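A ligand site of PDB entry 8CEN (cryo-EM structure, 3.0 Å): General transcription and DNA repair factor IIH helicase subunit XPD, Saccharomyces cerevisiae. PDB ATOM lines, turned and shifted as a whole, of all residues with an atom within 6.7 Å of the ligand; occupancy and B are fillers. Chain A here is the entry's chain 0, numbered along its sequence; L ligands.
Merely in contact with the ligand: Arg 111, His 117, Val 120, Tyr 158, His 159 and Phe 194.
11 residues have an atom within 4 Å of the ligand: Arg 111, Cys 115, Leu 116, His 117, Val 120, Cys 133, Cys 156, Tyr 158, His 159, Cys 191 and Phe 194.
The nearest printed residue that does not touch the ligand is Thr 137 (4.1 Å).
SG of Cys 191 lies close to N of Phe 194 (3.4 Å).
The backbone NH of Cys 191 is in hydrogen-bond range of the backbone carbonyl oxygen of Tyr 158 (3.3 Å).
The side-chain sulfur (SG) of Cys 115 lies close to the backbone carbonyl oxygen (O) of Val 120.
The side-chain sulfur (SG) of Cys 156 sits close to the backbone NH (N) of Tyr 158 (3.6 Å).
The guanidinium group (NE) of Arg 111 sits close to the side-chain sulfur (SG) of Cys 133 (3.0 Å).
The backbone carbonyl oxygen (O) of Leu 116 sits at hydrogen-bond distance from the side-chain hydroxyl (OH) of Tyr 158 (3.2 Å).
OH of Tyr 193 is in hydrogen-bond range of NH1 of Arg 111 (3.2 Å).
The side-chain carboxylate (OD1) of Asp 130 is in salt-bridge range of the guanidinium group (NH1) of Arg 111.
SG of Cys 191 binds FE4 of the ligand (2.3 Å).
An iron atom (FE1) of the ligand is bound by the side-chain sulfur (SG) of Cys 115 (2.3 Å).
An iron atom (FE2) of the ligand is bound by the side-chain sulfur (SG) of Cys 156, 2.3 Å away.
The side-chain sulfur of Cys 133 binds an iron atom (FE3) of the ligand, at 2.3 Å.
The backbone NH of Leu 116 lies close to a sulfur (S3) of the ligand, 3.7 Å away.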
ATOM      1  N   SER A 110      -3.621   5.389 -22.385  1.00  0.00           N
ATOM      2  CA  SER A 110      -3.459   4.379 -21.351  1.00  0.00           C
ATOM      3  C   SER A 110      -2.299   3.437 -21.661  1.00  0.00           C
ATOM      4  O   SER A 110      -1.659   3.508 -22.708  1.00  0.00           O
ATOM      5  CB  SER A 110      -4.757   3.600 -21.171  1.00  0.00           C
ATOM      6  OG  SER A 110      -5.084   2.871 -22.345  1.00  0.00           O
ATOM      7  N   ARG A 111      -2.043   2.535 -20.707  1.00  0.00           N
ATOM      8  CA  ARG A 111      -0.977   1.552 -20.845  1.00  0.00           C
ATOM      9  C   ARG A 111      -1.259   0.554 -21.960  1.00  0.00           C
ATOM     10  O   ARG A 111      -0.329   0.046 -22.594  1.00  0.00           O
ATOM     11  CB  ARG A 111      -0.777   0.804 -19.532  1.00  0.00           C
ATOM     12  CG  ARG A 111      -0.207   1.646 -18.405  1.00  0.00           C
ATOM     13  CD  ARG A 111      -0.092   0.800 -17.153  1.00  0.00           C
ATOM     14  NE  ARG A 111       0.750   1.406 -16.120  1.00  0.00           N
ATOM     15  CZ  ARG A 111       0.304   2.199 -15.160  1.00  0.00           C
ATOM     16  NH1 ARG A 111      -0.974   2.522 -15.057  1.00  0.00           N
ATOM     17  NH2 ARG A 111       1.176   2.685 -14.275  1.00  0.00           N
ATOM     18  N   LYS A 112      -2.542   0.251 -22.200  1.00  0.00           N
ATOM     19  CA  LYS A 112      -2.909  -0.665 -23.282  1.00  0.00           C
ATOM     20  C   LYS A 112      -2.504  -0.114 -24.640  1.00  0.00           C
ATOM     21  O   LYS A 112      -2.075  -0.866 -25.517  1.00  0.00           O
ATOM     22  CB  LYS A 112      -4.418  -0.940 -23.221  1.00  0.00           C
ATOM     23  CG  LYS A 112      -4.945  -1.810 -24.346  1.00  0.00           C
ATOM     24  CD  LYS A 112      -4.578  -3.269 -24.140  1.00  0.00           C
ATOM     25  CE  LYS A 112      -4.842  -4.083 -25.396  1.00  0.00           C
ATOM     26  NZ  LYS A 112      -4.396  -3.367 -26.628  1.00  0.00           N
ATOM     27  N   LEU A 114      -0.102   2.390 -24.949  1.00  0.00           N
ATOM     28  CA  LEU A 114       1.300   2.793 -24.899  1.00  0.00           C
ATOM     29  C   LEU A 114       2.162   1.754 -24.177  1.00  0.00           C
ATOM     30  O   LEU A 114       3.072   2.095 -23.422  1.00  0.00           O
ATOM     31  CB  LEU A 114       1.455   4.155 -24.226  1.00  0.00           C
ATOM     32  CG  LEU A 114       1.156   5.377 -25.098  1.00  0.00           C
ATOM     33  CD1 LEU A 114       1.348   6.657 -24.307  1.00  0.00           C
ATOM     34  CD2 LEU A 114       2.009   5.373 -26.349  1.00  0.00           C
ATOM     35  N   CYS A 115       1.892   0.473 -24.409  1.00  0.00           N
ATOM     36  CA  CYS A 115       2.695  -0.600 -23.858  1.00  0.00           C
ATOM     37  C   CYS A 115       3.453  -1.314 -24.971  1.00  0.00           C
ATOM     38  O   CYS A 115       2.856  -1.771 -25.939  1.00  0.00           O
ATOM     39  CB  CYS A 115       1.820  -1.605 -23.098  1.00  0.00           C
ATOM     40  SG  CYS A 115       2.745  -2.760 -22.056  1.00  0.00           S
ATOM     41  N   LEU A 116       4.781  -1.402 -24.812  1.00  0.00           N
ATOM     42  CA  LEU A 116       5.639  -2.124 -25.732  1.00  0.00           C
ATOM     43  C   LEU A 116       6.254  -3.378 -25.130  1.00  0.00           C
ATOM     44  O   LEU A 116       7.172  -3.947 -25.712  1.00  0.00           O
ATOM     45  CB  LEU A 116       6.745  -1.213 -26.265  1.00  0.00           C
ATOM     46  CG  LEU A 116       6.302  -0.046 -27.141  1.00  0.00           C
ATOM     47  CD1 LEU A 116       7.478   0.844 -27.467  1.00  0.00           C
ATOM     48  CD2 LEU A 116       5.695  -0.608 -28.418  1.00  0.00           C
ATOM     49  N   HIS A 117       5.777  -3.809 -23.970  1.00  0.00           N
ATOM     50  CA  HIS A 117       6.298  -5.027 -23.366  1.00  0.00           C
ATOM     51  C   HIS A 117       5.806  -6.238 -24.155  1.00  0.00           C
ATOM     52  O   HIS A 117       4.599  -6.364 -24.382  1.00  0.00           O
ATOM     53  CB  HIS A 117       5.887  -5.141 -21.902  1.00  0.00           C
ATOM     54  CG  HIS A 117       6.724  -6.102 -21.122  1.00  0.00           C
ATOM     55  ND1 HIS A 117       6.559  -7.464 -21.196  1.00  0.00           N
ATOM     56  CD2 HIS A 117       7.761  -5.889 -20.272  1.00  0.00           C
ATOM     57  CE1 HIS A 117       7.441  -8.063 -20.406  1.00  0.00           C
ATOM     58  NE2 HIS A 117       8.184  -7.131 -19.843  1.00  0.00           N
ATOM     59  N   VAL A 120       3.176  -8.595 -21.799  1.00  0.00           N
ATOM     60  CA  VAL A 120       1.870  -7.940 -21.586  1.00  0.00           C
ATOM     61  C   VAL A 120       1.642  -7.014 -22.781  1.00  0.00           C
ATOM     62  O   VAL A 120       1.785  -5.785 -22.724  1.00  0.00           O
ATOM     63  CB  VAL A 120       1.759  -7.297 -20.189  1.00  0.00           C
ATOM     64  CG1 VAL A 120       2.762  -6.146 -19.911  1.00  0.00           C
ATOM     65  CG2 VAL A 120       0.340  -6.827 -19.929  1.00  0.00           C
ATOM     66  N   VAL A 129      -3.699  -5.264 -18.138  1.00  0.00           N
ATOM     67  CA  VAL A 129      -2.444  -4.669 -18.602  1.00  0.00           C
ATOM     68  C   VAL A 129      -1.912  -3.689 -17.560  1.00  0.00           C
ATOM     69  O   VAL A 129      -0.707  -3.706 -17.217  1.00  0.00           O
ATOM     70  CB  VAL A 129      -2.624  -3.994 -19.966  1.00  0.00           C
ATOM     71  CG1 VAL A 129      -1.370  -3.246 -20.373  1.00  0.00           C
ATOM     72  CG2 VAL A 129      -2.962  -5.037 -21.026  1.00  0.00           C
ATOM     73  N   ASP A 130      -2.790  -2.850 -17.012  1.00  0.00           N
ATOM     74  CA  ASP A 130      -2.441  -1.929 -15.943  1.00  0.00           C
ATOM     75  C   ASP A 130      -1.913  -2.674 -14.719  1.00  0.00           C
ATOM     76  O   ASP A 130      -0.888  -2.299 -14.145  1.00  0.00           O
ATOM     77  CB  ASP A 130      -3.686  -1.102 -15.582  1.00  0.00           C
ATOM     78  CG  ASP A 130      -3.351   0.196 -14.882  1.00  0.00           C
ATOM     79  OD1 ASP A 130      -2.159   0.462 -14.676  1.00  0.00           O
ATOM     80  OD2 ASP A 130      -4.288   0.947 -14.553  1.00  0.00           O
ATOM     81  N   LYS A 132      -0.633  -5.771 -14.462  1.00  0.00           N
ATOM     82  CA  LYS A 132       0.672  -6.382 -14.700  1.00  0.00           C
ATOM     83  C   LYS A 132       1.780  -5.336 -14.765  1.00  0.00           C
ATOM     84  O   LYS A 132       2.903  -5.599 -14.299  1.00  0.00           O
ATOM     85  CB  LYS A 132       0.637  -7.224 -15.972  1.00  0.00           C
ATOM     86  CG  LYS A 132      -0.245  -8.450 -15.879  1.00  0.00           C
ATOM     87  CD  LYS A 132      -0.185  -9.287 -17.148  1.00  0.00           C
ATOM     88  CE  LYS A 132      -1.143 -10.465 -17.076  1.00  0.00           C
ATOM     89  NZ  LYS A 132      -0.729 -11.470 -16.048  1.00  0.00           N
ATOM     90  N   CYS A 133       1.481  -4.154 -15.307  1.00  0.00           N
ATOM     91  CA  CYS A 133       2.502  -3.109 -15.346  1.00  0.00           C
ATOM     92  C   CYS A 133       2.866  -2.622 -13.941  1.00  0.00           C
ATOM     93  O   CYS A 133       4.046  -2.444 -13.643  1.00  0.00           O
ATOM     94  CB  CYS A 133       2.036  -1.949 -16.207  1.00  0.00           C
ATOM     95  SG  CYS A 133       3.113  -0.502 -16.098  1.00  0.00           S
ATOM     96  N   ARG A 134       1.876  -2.428 -13.056  1.00  0.00           N
ATOM     97  CA  ARG A 134       2.226  -2.179 -11.658  1.00  0.00           C
ATOM     98  C   ARG A 134       2.913  -3.367 -10.997  1.00  0.00           C
ATOM     99  O   ARG A 134       3.891  -3.175 -10.274  1.00  0.00           O
ATOM    100  CB  ARG A 134       1.033  -1.729 -10.802  1.00  0.00           C
ATOM    101  CG  ARG A 134       0.601  -0.264 -10.961  1.00  0.00           C
ATOM    102  CD  ARG A 134      -0.266   0.012 -12.130  1.00  0.00           C
ATOM    103  NE  ARG A 134      -1.484  -0.785 -12.100  1.00  0.00           N
ATOM    104  CZ  ARG A 134      -2.579  -0.452 -11.430  1.00  0.00           C
ATOM    105  NH1 ARG A 134      -2.658   0.678 -10.744  1.00  0.00           N
ATOM    106  NH2 ARG A 134      -3.622  -1.278 -11.433  1.00  0.00           N
ATOM    107  N   MET A 136       4.962  -5.342 -12.194  1.00  0.00           N
ATOM    108  CA  MET A 136       6.367  -5.262 -12.544  1.00  0.00           C
ATOM    109  C   MET A 136       7.030  -3.937 -12.153  1.00  0.00           C
ATOM    110  O   MET A 136       8.266  -3.874 -12.132  1.00  0.00           O
ATOM    111  CB  MET A 136       6.534  -5.496 -14.041  1.00  0.00           C
ATOM    112  CG  MET A 136       6.160  -6.919 -14.451  1.00  0.00           C
ATOM    113  SD  MET A 136       6.241  -7.240 -16.221  1.00  0.00           S
ATOM    114  CE  MET A 136       8.000  -7.217 -16.483  1.00  0.00           C
ATOM    115  N   THR A 137       6.258  -2.871 -11.846  1.00  0.00           N
ATOM    116  CA  THR A 137       6.852  -1.542 -11.678  1.00  0.00           C
ATOM    117  C   THR A 137       6.363  -0.773 -10.447  1.00  0.00           C
ATOM    118  O   THR A 137       6.378   0.460 -10.482  1.00  0.00           O
ATOM    119  CB  THR A 137       6.600  -0.674 -12.920  1.00  0.00           C
ATOM    120  OG1 THR A 137       5.196  -0.496 -13.122  1.00  0.00           O
ATOM    121  CG2 THR A 137       7.227  -1.255 -14.183  1.00  0.00           C
ATOM    122  N   CYS A 156      10.369  -4.658 -15.903  1.00  0.00           N
ATOM    123  CA  CYS A 156      10.188  -4.247 -17.291  1.00  0.00           C
ATOM    124  C   CYS A 156      11.398  -3.427 -17.724  1.00  0.00           C
ATOM    125  O   CYS A 156      11.745  -2.433 -17.082  1.00  0.00           O
ATOM    126  CB  CYS A 156       8.892  -3.435 -17.440  1.00  0.00           C
ATOM    127  SG  CYS A 156       8.607  -2.744 -19.081  1.00  0.00           S
ATOM    128  N   GLU A 157      12.042  -3.864 -18.812  1.00  0.00           N
ATOM    129  CA  GLU A 157      13.258  -3.189 -19.266  1.00  0.00           C
ATOM    130  C   GLU A 157      12.954  -1.806 -19.817  1.00  0.00           C
ATOM    131  O   GLU A 157      13.800  -0.903 -19.703  1.00  0.00           O
ATOM    132  CB  GLU A 157      13.969  -4.041 -20.318  1.00  0.00           C
ATOM    133  CG  GLU A 157      13.176  -4.338 -21.581  1.00  0.00           C
ATOM    134  CD  GLU A 157      12.382  -5.635 -21.500  1.00  0.00           C
ATOM    135  OE1 GLU A 157      12.067  -6.069 -20.370  1.00  0.00           O
ATOM    136  OE2 GLU A 157      12.074  -6.218 -22.561  1.00  0.00           O
ATOM    137  N   TYR A 158      11.772  -1.607 -20.400  1.00  0.00           N
ATOM    138  CA  TYR A 158      11.381  -0.282 -20.894  1.00  0.00           C
ATOM    139  C   TYR A 158      11.237   0.711 -19.748  1.00  0.00           C
ATOM    140  O   TYR A 158      11.627   1.874 -19.868  1.00  0.00           O
ATOM    141  CB  TYR A 158      10.084  -0.383 -21.691  1.00  0.00           C
ATOM    142  CG  TYR A 158      10.165  -1.300 -22.890  1.00  0.00           C
ATOM    143  CD1 TYR A 158      10.601  -0.840 -24.117  1.00  0.00           C
ATOM    144  CD2 TYR A 158       9.800  -2.639 -22.788  1.00  0.00           C
ATOM    145  CE1 TYR A 158      10.684  -1.678 -25.217  1.00  0.00           C
ATOM    146  CE2 TYR A 158       9.864  -3.487 -23.881  1.00  0.00           C
ATOM    147  CZ  TYR A 158      10.311  -2.998 -25.091  1.00  0.00           C
ATOM    148  OH  TYR A 158      10.378  -3.835 -26.176  1.00  0.00           O
ATOM    149  N   HIS A 159      10.675   0.268 -18.619  1.00  0.00           N
ATOM    150  CA  HIS A 159      10.598   1.111 -17.441  1.00  0.00           C
ATOM    151  C   HIS A 159      11.973   1.295 -16.798  1.00  0.00           C
ATOM    152  O   HIS A 159      12.272   2.368 -16.267  1.00  0.00           O
ATOM    153  CB  HIS A 159       9.615   0.510 -16.438  1.00  0.00           C
ATOM    154  CG  HIS A 159       9.570   1.233 -15.123  1.00  0.00           C
ATOM    155  ND1 HIS A 159       8.951   2.448 -14.961  1.00  0.00           N
ATOM    156  CD2 HIS A 159      10.074   0.904 -13.909  1.00  0.00           C
ATOM    157  CE1 HIS A 159       9.066   2.834 -13.701  1.00  0.00           C
ATOM    158  NE2 HIS A 159       9.749   1.918 -13.049  1.00  0.00           N
ATOM    159  N   GLU A 160      12.814   0.249 -16.844  1.00  0.00           N
ATOM    160  CA  GLU A 160      14.113   0.310 -16.179  1.00  0.00           C
ATOM    161  C   GLU A 160      15.079   1.240 -16.909  1.00  0.00           C
ATOM    162  O   GLU A 160      15.916   1.881 -16.271  1.00  0.00           O
ATOM    163  CB  GLU A 160      14.703  -1.097 -16.074  1.00  0.00           C
ATOM    164  CG  GLU A 160      14.210  -1.877 -14.874  1.00  0.00           C
ATOM    165  CD  GLU A 160      14.116  -1.034 -13.616  1.00  0.00           C
ATOM    166  OE1 GLU A 160      15.169  -0.658 -13.065  1.00  0.00           O
ATOM    167  OE2 GLU A 160      12.975  -0.731 -13.188  1.00  0.00           O
ATOM    168  N   LEU A 190      12.367   2.039 -24.547  1.00  0.00           N
ATOM    169  CA  LEU A 190      11.857   2.905 -23.498  1.00  0.00           C
ATOM    170  C   LEU A 190      10.354   2.720 -23.380  1.00  0.00           C
ATOM    171  O   LEU A 190       9.709   2.195 -24.289  1.00  0.00           O
ATOM    172  CB  LEU A 190      12.181   4.390 -23.769  1.00  0.00           C
ATOM    173  CG  LEU A 190      13.617   4.763 -24.158  1.00  0.00           C
ATOM    174  CD1 LEU A 190      13.677   6.218 -24.609  1.00  0.00           C
ATOM    175  CD2 LEU A 190      14.561   4.537 -22.995  1.00  0.00           C
ATOM    176  N   CYS A 191       9.799   3.151 -22.249  1.00  0.00           N
ATOM    177  CA  CYS A 191       8.366   3.019 -22.016  1.00  0.00           C
ATOM    178  C   CYS A 191       7.667   4.305 -22.389  1.00  0.00           C
ATOM    179  O   CYS A 191       7.812   5.313 -21.671  1.00  0.00           O
ATOM    180  CB  CYS A 191       8.087   2.664 -20.560  1.00  0.00           C
ATOM    181  SG  CYS A 191       6.336   2.669 -20.154  1.00  0.00           S
ATOM    182  N   PRO A 192       6.891   4.336 -23.487  1.00  0.00           N
ATOM    183  CA  PRO A 192       6.231   5.586 -23.895  1.00  0.00           C
ATOM    184  C   PRO A 192       5.216   6.094 -22.901  1.00  0.00           C
ATOM    185  O   PRO A 192       5.096   7.311 -22.724  1.00  0.00           O
ATOM    186  CB  PRO A 192       5.572   5.202 -25.224  1.00  0.00           C
ATOM    187  CG  PRO A 192       5.409   3.722 -25.168  1.00  0.00           C
ATOM    188  CD  PRO A 192       6.564   3.206 -24.364  1.00  0.00           C
ATOM    189  N   TYR A 193       4.491   5.197 -22.225  1.00  0.00           N
ATOM    190  CA  TYR A 193       3.482   5.602 -21.248  1.00  0.00           C
ATOM    191  C   TYR A 193       4.117   6.364 -20.089  1.00  0.00           C
ATOM    192  O   TYR A 193       3.699   7.476 -19.763  1.00  0.00           O
ATOM    193  CB  TYR A 193       2.744   4.359 -20.738  1.00  0.00           C
ATOM    194  CG  TYR A 193       1.834   4.632 -19.566  1.00  0.00           C
ATOM    195  CD1 TYR A 193       0.589   5.228 -19.759  1.00  0.00           C
ATOM    196  CD2 TYR A 193       2.225   4.327 -18.265  1.00  0.00           C
ATOM    197  CE1 TYR A 193      -0.245   5.473 -18.693  1.00  0.00           C
ATOM    198  CE2 TYR A 193       1.394   4.596 -17.197  1.00  0.00           C
ATOM    199  CZ  TYR A 193       0.160   5.155 -17.416  1.00  0.00           C
ATOM    200  OH  TYR A 193      -0.678   5.417 -16.348  1.00  0.00           O
ATOM    201  N   PHE A 194       5.141   5.774 -19.477  1.00  0.00           N
ATOM    202  CA  PHE A 194       5.808   6.423 -18.366  1.00  0.00           C
ATOM    203  C   PHE A 194       6.605   7.647 -18.817  1.00  0.00           C
ATOM    204  O   PHE A 194       6.773   8.587 -18.034  1.00  0.00           O
ATOM    205  CB  PHE A 194       6.714   5.438 -17.634  1.00  0.00           C
ATOM    206  CG  PHE A 194       6.017   4.679 -16.542  1.00  0.00           C
ATOM    207  CD1 PHE A 194       5.701   5.294 -15.342  1.00  0.00           C
ATOM    208  CD2 PHE A 194       5.668   3.348 -16.717  1.00  0.00           C
ATOM    209  CE1 PHE A 194       5.056   4.600 -14.332  1.00  0.00           C
ATOM    210  CE2 PHE A 194       5.027   2.650 -15.714  1.00  0.00           C
ATOM    211  CZ  PHE A 194       4.724   3.280 -14.528  1.00  0.00           C
HETATM  212 FE1  LIG L   1       4.163  -1.724 -20.618  1.00  0.00          FE
HETATM  213 FE2  LIG L   1       6.528  -1.837 -19.248  1.00  0.00          FE
HETATM  214 FE3  LIG L   1       4.272  -0.906 -18.015  1.00  0.00          FE
HETATM  215 FE4  LIG L   1       5.472   0.582 -19.965  1.00  0.00          FE
HETATM  216  S1  LIG L   1       6.350   0.024 -17.940  1.00  0.00           S
HETATM  217  S2  LIG L   1       3.244   0.165 -19.742  1.00  0.00           S
HETATM  218  S3  LIG L   1       6.212  -1.056 -21.369  1.00  0.00           S
HETATM  219  S4  LIG L   1       4.630  -3.020 -18.795  1.00  0.00           S
